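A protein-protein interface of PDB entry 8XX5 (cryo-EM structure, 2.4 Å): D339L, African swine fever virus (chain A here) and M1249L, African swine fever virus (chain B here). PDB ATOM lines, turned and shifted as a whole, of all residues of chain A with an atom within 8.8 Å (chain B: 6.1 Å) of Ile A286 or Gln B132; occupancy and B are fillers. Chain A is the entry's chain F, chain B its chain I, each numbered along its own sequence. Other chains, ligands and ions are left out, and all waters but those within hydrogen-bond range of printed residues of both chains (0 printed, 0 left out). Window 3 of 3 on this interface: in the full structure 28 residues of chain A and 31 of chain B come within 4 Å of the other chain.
The backbone carbonyl oxygen (O) of Pro A284 sits at hydrogen-bond distance from a ring nitrogen (NE2) of His B135 (3.3 Å).
O of Ile A286 sits at hydrogen-bond distance from NE2 of Gln B136.
N of His A165 lies within hydrogen-bond range of O of Ile A285 (2.9 Å).
N of Cys A287 is in hydrogen-bond range of O of His A165, at 2.8 Å.
N of Gln A167 sits at hydrogen-bond distance from O of Cys A287 (3.2 Å).
The backbone carbonyl oxygen of Glu A168 sits at hydrogen-bond distance from the backbone NH of Ala A289.
OG of Ser A288 sits close to N of Val A291, 3.5 Å away.
The side-chain sulfur (SG) of Cys B109 lies within hydrogen-bond range of the side-chain amide nitrogen (NE2) of Gln B136, 3.6 Å away.
Printed residues of chain A that touch a printed residue of chain B: Glu A168, Leu A283, Pro A284, Ile A285, Ile A286, Cys A287, Ser A288 and Val A291.
Hydrophobic or aromatic side chains of chain A within 4 Å of the printed part of chain B: Ile A285, Ile A286 and Val A291.
Among the printed residues, 12 pairs touch across the chains.
Among the printed residues, merely in contact across the chains: Glu A168 with Val B105 (3.2 Å), Leu A283 with His B135 (3.6 Å), Ile A285 with Phe B106 (3.6 Å), Ile A286 with Phe B106 (3.8 Å), Ile A286 with Cys B109 (3.6 Å), Ile A286 with Gln B132 (3.3 Å), Cys A287 with Val B105 (3.8 Å), Cys A287 with Phe B106 (3.9 Å), Ser A288 with Val B105 (3.3 Å) and Val A291 with Phe B106 (3.6 Å).
Of chain B, only Phe B106, Cys B109, Gln B132 and Gln B136 come within 4 Å of Ile A286.
Of chain A, only Ile A286 comes within 4 Å of Gln B132.
Of the printed residues of chain A, His B135 touches Leu A283 and Pro A284.
Of the printed residues of chain B, Glu A168 touches Val B105 (3.2 Å).
Of the printed residues of chain A, Val B105 touches Glu A168, Cys A287 and Ser A288.
Phe B133 touches none of the printed residues of chain A.
Met B107 touches none of the printed residues of chain A.
The nearest residue of chain B that does not touch Ile A286 is Val B105 (4.4 Å).
The nearest residue of chain A that does not touch Gln B132 is Leu A283 (5.1 Å).
The nearest printed residue of chain B that does not touch Pro A284 is Gln B136 (4.1 Å).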
ATOM      1  N   VAL A 163      33.139  -0.751  24.774  1.00  0.00           N
ATOM      2  CA  VAL A 163      33.436  -1.890  23.913  1.00  0.00           C
ATOM      3  C   VAL A 163      32.331  -1.994  22.872  1.00  0.00           C
ATOM      4  O   VAL A 163      31.144  -1.977  23.218  1.00  0.00           O
ATOM      5  CB  VAL A 163      33.558  -3.192  24.721  1.00  0.00           C
ATOM      6  CG1 VAL A 163      34.013  -4.333  23.829  1.00  0.00           C
ATOM      7  CG2 VAL A 163      34.520  -3.006  25.884  1.00  0.00           C
ATOM      8  N   TYR A 164      32.718  -2.102  21.605  1.00  0.00           N
ATOM      9  CA  TYR A 164      31.775  -2.097  20.492  1.00  0.00           C
ATOM     10  C   TYR A 164      31.730  -3.487  19.869  1.00  0.00           C
ATOM     11  O   TYR A 164      32.745  -3.986  19.373  1.00  0.00           O
ATOM     12  CB  TYR A 164      32.167  -1.046  19.456  1.00  0.00           C
ATOM     13  CG  TYR A 164      31.783   0.359  19.851  1.00  0.00           C
ATOM     14  CD1 TYR A 164      32.603   1.116  20.677  1.00  0.00           C
ATOM     15  CD2 TYR A 164      30.600   0.928  19.403  1.00  0.00           C
ATOM     16  CE1 TYR A 164      32.256   2.399  21.046  1.00  0.00           C
ATOM     17  CE2 TYR A 164      30.244   2.210  19.766  1.00  0.00           C
ATOM     18  CZ  TYR A 164      31.076   2.942  20.589  1.00  0.00           C
ATOM     19  OH  TYR A 164      30.725   4.221  20.952  1.00  0.00           O
ATOM     20  N   HIS A 165      30.552  -4.105  19.897  1.00  0.00           N
ATOM     21  CA  HIS A 165      30.338  -5.371  19.212  1.00  0.00           C
ATOM     22  C   HIS A 165      29.830  -5.099  17.803  1.00  0.00           C
ATOM     23  O   HIS A 165      28.842  -4.383  17.618  1.00  0.00           O
ATOM     24  CB  HIS A 165      29.344  -6.235  19.989  1.00  0.00           C
ATOM     25  CG  HIS A 165      29.166  -7.612  19.427  1.00  0.00           C
ATOM     26  ND1 HIS A 165      29.978  -8.127  18.439  1.00  0.00           N
ATOM     27  CD2 HIS A 165      28.269  -8.583  19.720  1.00  0.00           C
ATOM     28  CE1 HIS A 165      29.588  -9.355  18.146  1.00  0.00           C
ATOM     29  NE2 HIS A 165      28.552  -9.656  18.910  1.00  0.00           N
ATOM     30  N   VAL A 166      30.507  -5.667  16.809  1.00  0.00           N
ATOM     31  CA  VAL A 166      30.222  -5.399  15.404  1.00  0.00           C
ATOM     32  C   VAL A 166      29.665  -6.667  14.776  1.00  0.00           C
ATOM     33  O   VAL A 166      30.350  -7.696  14.727  1.00  0.00           O
ATOM     34  CB  VAL A 166      31.474  -4.920  14.654  1.00  0.00           C
ATOM     35  CG1 VAL A 166      31.206  -4.860  13.163  1.00  0.00           C
ATOM     36  CG2 VAL A 166      31.910  -3.564  15.178  1.00  0.00           C
ATOM     37  N   GLN A 167      28.427  -6.592  14.290  1.00  0.00           N
ATOM     38  CA  GLN A 167      27.767  -7.719  13.649  1.00  0.00           C
ATOM     39  C   GLN A 167      27.453  -7.472  12.181  1.00  0.00           C
ATOM     40  O   GLN A 167      27.020  -8.403  11.492  1.00  0.00           O
ATOM     41  CB  GLN A 167      26.479  -8.076  14.398  1.00  0.00           C
ATOM     42  CG  GLN A 167      26.674  -8.344  15.878  1.00  0.00           C
ATOM     43  CD  GLN A 167      25.483  -9.045  16.501  1.00  0.00           C
ATOM     44  OE1 GLN A 167      24.708  -9.707  15.810  1.00  0.00           O
ATOM     45  NE2 GLN A 167      25.335  -8.909  17.813  1.00  0.00           N
ATOM     46  N   GLU A 168      27.656  -6.257  11.682  1.00  0.00           N
ATOM     47  CA  GLU A 168      27.387  -5.919  10.291  1.00  0.00           C
ATOM     48  C   GLU A 168      28.697  -5.582   9.594  1.00  0.00           C
ATOM     49  O   GLU A 168      29.513  -4.825  10.127  1.00  0.00           O
ATOM     50  CB  GLU A 168      26.406  -4.749  10.183  1.00  0.00           C
ATOM     51  CG  GLU A 168      26.486  -3.994   8.866  1.00  0.00           C
ATOM     52  CD  GLU A 168      25.151  -3.416   8.443  1.00  0.00           C
ATOM     53  OE1 GLU A 168      24.196  -3.478   9.245  1.00  0.00           O
ATOM     54  OE2 GLU A 168      25.055  -2.899   7.310  1.00  0.00           O
ATOM     55  N   GLY A 255      33.240  -8.970  14.726  1.00  0.00           N
ATOM     56  CA  GLY A 255      33.876  -9.287  15.989  1.00  0.00           C
ATOM     57  C   GLY A 255      33.596  -8.268  17.074  1.00  0.00           C
ATOM     58  O   GLY A 255      32.573  -7.580  17.037  1.00  0.00           O
ATOM     59  N   PHE A 256      34.497  -8.168  18.046  1.00  0.00           N
ATOM     60  CA  PHE A 256      34.383  -7.216  19.142  1.00  0.00           C
ATOM     61  C   PHE A 256      35.486  -6.174  19.032  1.00  0.00           C
ATOM     62  O   PHE A 256      36.601  -6.479  18.600  1.00  0.00           O
ATOM     63  CB  PHE A 256      34.462  -7.919  20.501  1.00  0.00           C
ATOM     64  CG  PHE A 256      33.265  -8.771  20.819  1.00  0.00           C
ATOM     65  CD1 PHE A 256      33.005  -9.930  20.108  1.00  0.00           C
ATOM     66  CD2 PHE A 256      32.399  -8.408  21.836  1.00  0.00           C
ATOM     67  CE1 PHE A 256      31.904 -10.710  20.404  1.00  0.00           C
ATOM     68  CE2 PHE A 256      31.298  -9.184  22.136  1.00  0.00           C
ATOM     69  CZ  PHE A 256      31.050 -10.335  21.420  1.00  0.00           C
ATOM     70  N   GLU A 282      30.541  -2.350  31.310  1.00  0.00           N
ATOM     71  CA  GLU A 282      29.426  -1.973  30.456  1.00  0.00           C
ATOM     72  C   GLU A 282      29.263  -3.023  29.369  1.00  0.00           C
ATOM     73  O   GLU A 282      30.246  -3.599  28.893  1.00  0.00           O
ATOM     74  CB  GLU A 282      29.637  -0.587  29.836  1.00  0.00           C
ATOM     75  CG  GLU A 282      31.049  -0.349  29.328  1.00  0.00           C
ATOM     76  CD  GLU A 282      31.185  -0.615  27.843  1.00  0.00           C
ATOM     77  OE1 GLU A 282      30.212  -0.359  27.101  1.00  0.00           O
ATOM     78  OE2 GLU A 282      32.260  -1.086  27.418  1.00  0.00           O
ATOM     79  N   LEU A 283      28.014  -3.264  28.984  1.00  0.00           N
ATOM     80  CA  LEU A 283      27.728  -4.256  27.962  1.00  0.00           C
ATOM     81  C   LEU A 283      28.241  -3.784  26.602  1.00  0.00           C
ATOM     82  O   LEU A 283      28.293  -2.582  26.332  1.00  0.00           O
ATOM     83  CB  LEU A 283      26.229  -4.530  27.888  1.00  0.00           C
ATOM     84  CG  LEU A 283      25.648  -5.410  28.994  1.00  0.00           C
ATOM     85  CD1 LEU A 283      24.303  -4.873  29.455  1.00  0.00           C
ATOM     86  CD2 LEU A 283      25.521  -6.849  28.520  1.00  0.00           C
ATOM     87  N   PRO A 284      28.641  -4.713  25.734  1.00  0.00           N
ATOM     88  CA  PRO A 284      29.098  -4.320  24.396  1.00  0.00           C
ATOM     89  C   PRO A 284      27.993  -3.630  23.612  1.00  0.00           C
ATOM     90  O   PRO A 284      26.817  -3.986  23.708  1.00  0.00           O
ATOM     91  CB  PRO A 284      29.500  -5.652  23.750  1.00  0.00           C
ATOM     92  CG  PRO A 284      29.724  -6.583  24.893  1.00  0.00           C
ATOM     93  CD  PRO A 284      28.759  -6.163  25.954  1.00  0.00           C
ATOM     94  N   ILE A 285      28.386  -2.630  22.826  1.00  0.00           N
ATOM     95  CA  ILE A 285      27.452  -1.849  22.024  1.00  0.00           C
ATOM     96  C   ILE A 285      27.328  -2.547  20.675  1.00  0.00           C
ATOM     97  O   ILE A 285      28.201  -2.424  19.814  1.00  0.00           O
ATOM     98  CB  ILE A 285      27.913  -0.400  21.873  1.00  0.00           C
ATOM     99  CG1 ILE A 285      28.013   0.272  23.244  1.00  0.00           C
ATOM    100  CG2 ILE A 285      26.966   0.367  20.969  1.00  0.00           C
ATOM    101  CD1 ILE A 285      29.031   1.386  23.303  1.00  0.00           C
ATOM    102  N   ILE A 286      26.238  -3.289  20.489  1.00  0.00           N
ATOM    103  CA  ILE A 286      26.014  -3.983  19.228  1.00  0.00           C
ATOM    104  C   ILE A 286      25.680  -2.954  18.157  1.00  0.00           C
ATOM    105  O   ILE A 286      24.702  -2.206  18.275  1.00  0.00           O
ATOM    106  CB  ILE A 286      24.901  -5.029  19.362  1.00  0.00           C
ATOM    107  CG1 ILE A 286      25.302  -6.109  20.367  1.00  0.00           C
ATOM    108  CG2 ILE A 286      24.598  -5.648  18.010  1.00  0.00           C
ATOM    109  CD1 ILE A 286      24.641  -5.961  21.717  1.00  0.00           C
ATOM    110  N   CYS A 287      26.491  -2.911  17.108  1.00  0.00           N
ATOM    111  CA  CYS A 287      26.330  -1.928  16.045  1.00  0.00           C
ATOM    112  C   CYS A 287      26.974  -2.484  14.782  1.00  0.00           C
ATOM    113  O   CYS A 287      27.306  -3.672  14.706  1.00  0.00           O
ATOM    114  CB  CYS A 287      26.930  -0.579  16.457  1.00  0.00           C
ATOM    115  SG  CYS A 287      28.697  -0.627  16.827  1.00  0.00           S
ATOM    116  N   SER A 288      27.139  -1.626  13.783  1.00  0.00           N
ATOM    117  CA  SER A 288      27.750  -2.016  12.525  1.00  0.00           C
ATOM    118  C   SER A 288      29.227  -1.638  12.511  1.00  0.00           C
ATOM    119  O   SER A 288      29.729  -0.940  13.393  1.00  0.00           O
ATOM    120  CB  SER A 288      27.025  -1.362  11.350  1.00  0.00           C
ATOM    121  OG  SER A 288      27.049   0.050  11.457  1.00  0.00           O
ATOM    122  N   ALA A 289      29.928  -2.116  11.481  1.00  0.00           N
ATOM    123  CA  ALA A 289      31.328  -1.748  11.317  1.00  0.00           C
ATOM    124  C   ALA A 289      31.484  -0.253  11.087  1.00  0.00           C
ATOM    125  O   ALA A 289      32.452   0.349  11.563  1.00  0.00           O
ATOM    126  CB  ALA A 289      31.946  -2.534  10.162  1.00  0.00           C
ATOM    127  N   VAL A 291      29.615   2.226  12.289  1.00  0.00           N
ATOM    128  CA  VAL A 291      29.436   2.977  13.529  1.00  0.00           C
ATOM    129  C   VAL A 291      30.704   2.918  14.373  1.00  0.00           C
ATOM    130  O   VAL A 291      31.208   3.945  14.846  1.00  0.00           O
ATOM    131  CB  VAL A 291      28.220   2.444  14.307  1.00  0.00           C
ATOM    132  CG1 VAL A 291      28.156   3.073  15.688  1.00  0.00           C
ATOM    133  CG2 VAL A 291      26.939   2.703  13.532  1.00  0.00           C
ATOM    134  N   MET A 292      31.241   1.711  14.564  1.00  0.00           N
ATOM    135  CA  MET A 292      32.451   1.555  15.365  1.00  0.00           C
ATOM    136  C   MET A 292      33.633   2.270  14.729  1.00  0.00           C
ATOM    137  O   MET A 292      34.406   2.944  15.421  1.00  0.00           O
ATOM    138  CB  MET A 292      32.769   0.073  15.555  1.00  0.00           C
ATOM    139  CG  MET A 292      34.103  -0.189  16.240  1.00  0.00           C
ATOM    140  SD  MET A 292      35.457  -0.449  15.077  1.00  0.00           S
ATOM    141  CE  MET A 292      34.717  -1.610  13.935  1.00  0.00           C
ATOM    142  N   VAL B 105      20.511  -0.524  12.385  1.00  0.00           N
ATOM    143  CA  VAL B 105      21.756  -1.188  12.757  1.00  0.00           C
ATOM    144  C   VAL B 105      21.800  -1.427  14.260  1.00  0.00           C
ATOM    145  O   VAL B 105      22.168  -2.514  14.723  1.00  0.00           O
ATOM    146  CB  VAL B 105      22.965  -0.363  12.273  1.00  0.00           C
ATOM    147  CG1 VAL B 105      24.104  -0.418  13.279  1.00  0.00           C
ATOM    148  CG2 VAL B 105      23.421  -0.842  10.905  1.00  0.00           C
ATOM    149  N   PHE B 106      21.411  -0.422  15.045  1.00  0.00           N
ATOM    150  CA  PHE B 106      21.481  -0.527  16.495  1.00  0.00           C
ATOM    151  C   PHE B 106      20.366  -1.389  17.071  1.00  0.00           C
ATOM    152  O   PHE B 106      20.569  -2.040  18.102  1.00  0.00           O
ATOM    153  CB  PHE B 106      21.421   0.864  17.127  1.00  0.00           C
ATOM    154  CG  PHE B 106      22.766   1.492  17.352  1.00  0.00           C
ATOM    155  CD1 PHE B 106      23.396   2.194  16.341  1.00  0.00           C
ATOM    156  CD2 PHE B 106      23.395   1.388  18.581  1.00  0.00           C
ATOM    157  CE1 PHE B 106      24.630   2.777  16.549  1.00  0.00           C
ATOM    158  CE2 PHE B 106      24.628   1.968  18.794  1.00  0.00           C
ATOM    159  CZ  PHE B 106      25.246   2.662  17.777  1.00  0.00           C
ATOM    160  N   MET B 107      19.191  -1.404  16.440  1.00  0.00           N
ATOM    161  CA  MET B 107      18.001  -1.944  17.081  1.00  0.00           C
ATOM    162  C   MET B 107      17.516  -3.273  16.519  1.00  0.00           C
ATOM    163  O   MET B 107      16.733  -3.953  17.191  1.00  0.00           O
ATOM    164  CB  MET B 107      16.858  -0.926  16.995  1.00  0.00           C
ATOM    165  CG  MET B 107      16.145  -0.715  18.305  1.00  0.00           C
ATOM    166  SD  MET B 107      17.095   0.359  19.390  1.00  0.00           S
ATOM    167  CE  MET B 107      16.037   0.363  20.824  1.00  0.00           C
ATOM    168  N   CYS B 109      19.085  -5.950  16.267  1.00  0.00           N
ATOM    169  CA  CYS B 109      19.701  -7.037  17.015  1.00  0.00           C
ATOM    170  C   CYS B 109      18.859  -7.501  18.196  1.00  0.00           C
ATOM    171  O   CYS B 109      19.177  -8.535  18.794  1.00  0.00           O
ATOM    172  CB  CYS B 109      21.080  -6.606  17.515  1.00  0.00           C
ATOM    173  SG  CYS B 109      21.048  -5.178  18.626  1.00  0.00           S
ATOM    174  N   VAL B 110      17.805  -6.769  18.547  1.00  0.00           N
ATOM    175  CA  VAL B 110      16.963  -7.119  19.686  1.00  0.00           C
ATOM    176  C   VAL B 110      15.523  -7.263  19.199  1.00  0.00           C
ATOM    177  O   VAL B 110      14.566  -6.989  19.931  1.00  0.00           O
ATOM    178  CB  VAL B 110      17.120  -6.074  20.813  1.00  0.00           C
ATOM    179  CG1 VAL B 110      16.495  -4.731  20.433  1.00  0.00           C
ATOM    180  CG2 VAL B 110      16.592  -6.603  22.145  1.00  0.00           C
ATOM    181  N   LYS B 127      11.838  -9.578  29.677  1.00  0.00           N
ATOM    182  CA  LYS B 127      12.439  -8.515  30.477  1.00  0.00           C
ATOM    183  C   LYS B 127      13.887  -8.264  30.074  1.00  0.00           C
ATOM    184  O   LYS B 127      14.295  -7.115  29.867  1.00  0.00           O
ATOM    185  CB  LYS B 127      12.342  -8.857  31.964  1.00  0.00           C
ATOM    186  CG  LYS B 127      12.948  -7.805  32.874  1.00  0.00           C
ATOM    187  CD  LYS B 127      12.330  -7.841  34.260  1.00  0.00           C
ATOM    188  CE  LYS B 127      12.147  -6.437  34.805  1.00  0.00           C
ATOM    189  NZ  LYS B 127      11.649  -5.499  33.760  1.00  0.00           N
ATOM    190  N   GLU B 128      14.681  -9.330  29.947  1.00  0.00           N
ATOM    191  CA  GLU B 128      16.071  -9.164  29.530  1.00  0.00           C
ATOM    192  C   GLU B 128      16.148  -8.526  28.149  1.00  0.00           C
ATOM    193  O   GLU B 128      17.047  -7.718  27.875  1.00  0.00           O
ATOM    194  CB  GLU B 128      16.790 -10.513  29.551  1.00  0.00           C
ATOM    195  CG  GLU B 128      15.983 -11.660  28.969  1.00  0.00           C
ATOM    196  CD  GLU B 128      16.291 -11.909  27.506  1.00  0.00           C
ATOM    197  OE1 GLU B 128      17.480 -11.839  27.129  1.00  0.00           O
ATOM    198  OE2 GLU B 128      15.346 -12.174  26.734  1.00  0.00           O
ATOM    199  N   ASN B 129      15.200  -8.865  27.273  1.00  0.00           N
ATOM    200  CA  ASN B 129      15.094  -8.168  25.999  1.00  0.00           C
ATOM    201  C   ASN B 129      14.786  -6.692  26.201  1.00  0.00           C
ATOM    202  O   ASN B 129      15.255  -5.856  25.427  1.00  0.00           O
ATOM    203  CB  ASN B 129      14.024  -8.819  25.125  1.00  0.00           C
ATOM    204  CG  ASN B 129      14.588  -9.892  24.218  1.00  0.00           C
ATOM    205  OD1 ASN B 129      14.249 -11.067  24.344  1.00  0.00           O
ATOM    206  ND2 ASN B 129      15.458  -9.493  23.300  1.00  0.00           N
ATOM    207  N   ILE B 130      14.016  -6.350  27.237  1.00  0.00           N
ATOM    208  CA  ILE B 130      13.740  -4.943  27.519  1.00  0.00           C
ATOM    209  C   ILE B 130      15.013  -4.221  27.949  1.00  0.00           C
ATOM    210  O   ILE B 130      15.274  -3.091  27.519  1.00  0.00           O
ATOM    211  CB  ILE B 130      12.629  -4.814  28.579  1.00  0.00           C
ATOM    212  CG1 ILE B 130      11.289  -5.303  28.020  1.00  0.00           C
ATOM    213  CG2 ILE B 130      12.527  -3.380  29.072  1.00  0.00           C
ATOM    214  CD1 ILE B 130      10.411  -4.206  27.451  1.00  0.00           C
ATOM    215  N   ILE B 131      15.821  -4.851  28.809  1.00  0.00           N
ATOM    216  CA  ILE B 131      17.087  -4.234  29.212  1.00  0.00           C
ATOM    217  C   ILE B 131      18.000  -4.042  28.007  1.00  0.00           C
ATOM    218  O   ILE B 131      18.608  -2.976  27.832  1.00  0.00           O
ATOM    219  CB  ILE B 131      17.783  -5.059  30.316  1.00  0.00           C
ATOM    220  CG1 ILE B 131      17.061  -4.919  31.661  1.00  0.00           C
ATOM    221  CG2 ILE B 131      19.243  -4.653  30.452  1.00  0.00           C
ATOM    222  CD1 ILE B 131      16.125  -6.041  32.003  1.00  0.00           C
ATOM    223  N   GLN B 132      18.115  -5.067  27.158  1.00  0.00           N
ATOM    224  CA  GLN B 132      18.955  -4.947  25.970  1.00  0.00           C
ATOM    225  C   GLN B 132      18.433  -3.862  25.033  1.00  0.00           C
ATOM    226  O   GLN B 132      19.214  -3.095  24.460  1.00  0.00           O
ATOM    227  CB  GLN B 132      19.035  -6.292  25.250  1.00  0.00           C
ATOM    228  CG  GLN B 132      19.718  -6.237  23.896  1.00  0.00           C
ATOM    229  CD  GLN B 132      21.144  -6.740  23.947  1.00  0.00           C
ATOM    230  OE1 GLN B 132      21.749  -6.811  25.016  1.00  0.00           O
ATOM    231  NE2 GLN B 132      21.685  -7.106  22.792  1.00  0.00           N
ATOM    232  N   PHE B 133      17.111  -3.787  24.872  1.00  0.00           N
ATOM    233  CA  PHE B 133      16.494  -2.768  24.031  1.00  0.00           C
ATOM    234  C   PHE B 133      16.812  -1.373  24.549  1.00  0.00           C
ATOM    235  O   PHE B 133      17.184  -0.482  23.778  1.00  0.00           O
ATOM    236  CB  PHE B 133      14.984  -3.016  23.992  1.00  0.00           C
ATOM    237  CG  PHE B 133      14.199  -2.001  23.210  1.00  0.00           C
ATOM    238  CD1 PHE B 133      13.774  -0.821  23.800  1.00  0.00           C
ATOM    239  CD2 PHE B 133      13.834  -2.256  21.899  1.00  0.00           C
ATOM    240  CE1 PHE B 133      13.038   0.102  23.086  1.00  0.00           C
ATOM    241  CE2 PHE B 133      13.092  -1.339  21.182  1.00  0.00           C
ATOM    242  CZ  PHE B 133      12.695  -0.158  21.775  1.00  0.00           C
ATOM    243  N   THR B 134      16.680  -1.170  25.861  1.00  0.00           N
ATOM    244  CA  THR B 134      16.977   0.135  26.443  1.00  0.00           C
ATOM    245  C   THR B 134      18.448   0.494  26.269  1.00  0.00           C
ATOM    246  O   THR B 134      18.778   1.632  25.913  1.00  0.00           O
ATOM    247  CB  THR B 134      16.594   0.153  27.921  1.00  0.00           C
ATOM    248  OG1 THR B 134      15.169   0.229  28.047  1.00  0.00           O
ATOM    249  CG2 THR B 134      17.221   1.347  28.619  1.00  0.00           C
ATOM    250  N   HIS B 135      19.346  -0.464  26.508  1.00  0.00           N
ATOM    251  CA  HIS B 135      20.772  -0.191  26.358  1.00  0.00           C
ATOM    252  C   HIS B 135      21.108   0.177  24.918  1.00  0.00           C
ATOM    253  O   HIS B 135      21.847   1.137  24.662  1.00  0.00           O
ATOM    254  CB  HIS B 135      21.589  -1.402  26.815  1.00  0.00           C
ATOM    255  CG  HIS B 135      23.001  -1.405  26.316  1.00  0.00           C
ATOM    256  ND1 HIS B 135      23.985  -0.606  26.858  1.00  0.00           N
ATOM    257  CD2 HIS B 135      23.595  -2.118  25.330  1.00  0.00           C
ATOM    258  CE1 HIS B 135      25.123  -0.823  26.224  1.00  0.00           C
ATOM    259  NE2 HIS B 135      24.914  -1.735  25.293  1.00  0.00           N
ATOM    260  N   GLN B 136      20.557  -0.574  23.961  1.00  0.00           N
ATOM    261  CA  GLN B 136      20.805  -0.283  22.555  1.00  0.00           C
ATOM    262  C   GLN B 136      20.238   1.072  22.164  1.00  0.00           C
ATOM    263  O   GLN B 136      20.847   1.800  21.376  1.00  0.00           O
ATOM    264  CB  GLN B 136      20.219  -1.388  21.678  1.00  0.00           C
ATOM    265  CG  GLN B 136      20.989  -2.692  21.738  1.00  0.00           C
ATOM    266  CD  GLN B 136      22.398  -2.560  21.199  1.00  0.00           C
ATOM    267  OE1 GLN B 136      23.372  -2.802  21.910  1.00  0.00           O
ATOM    268  NE2 GLN B 136      22.514  -2.177  19.933  1.00  0.00           N
ATOM    269  N   TYR B 137      19.069   1.429  22.701  1.00  0.00           N
ATOM    270  CA  TYR B 137      18.484   2.731  22.399  1.00  0.00           C
ATOM    271  C   TYR B 137      19.360   3.857  22.930  1.00  0.00           C
ATOM    272  O   TYR B 137      19.596   4.856  22.237  1.00  0.00           O
ATOM    273  CB  TYR B 137      17.082   2.817  22.998  1.00  0.00           C
ATOM    274  CG  TYR B 137      16.327   4.074  22.647  1.00  0.00           C
ATOM    275  CD1 TYR B 137      16.479   5.236  23.390  1.00  0.00           C
ATOM    276  CD2 TYR B 137      15.452   4.094  21.570  1.00  0.00           C
ATOM    277  CE1 TYR B 137      15.785   6.380  23.068  1.00  0.00           C
ATOM    278  CE2 TYR B 137      14.755   5.230  21.242  1.00  0.00           C
ATOM    279  CZ  TYR B 137      14.925   6.370  21.994  1.00  0.00           C
ATOM    280  OH  TYR B 137      14.233   7.509  21.669  1.00  0.00           O
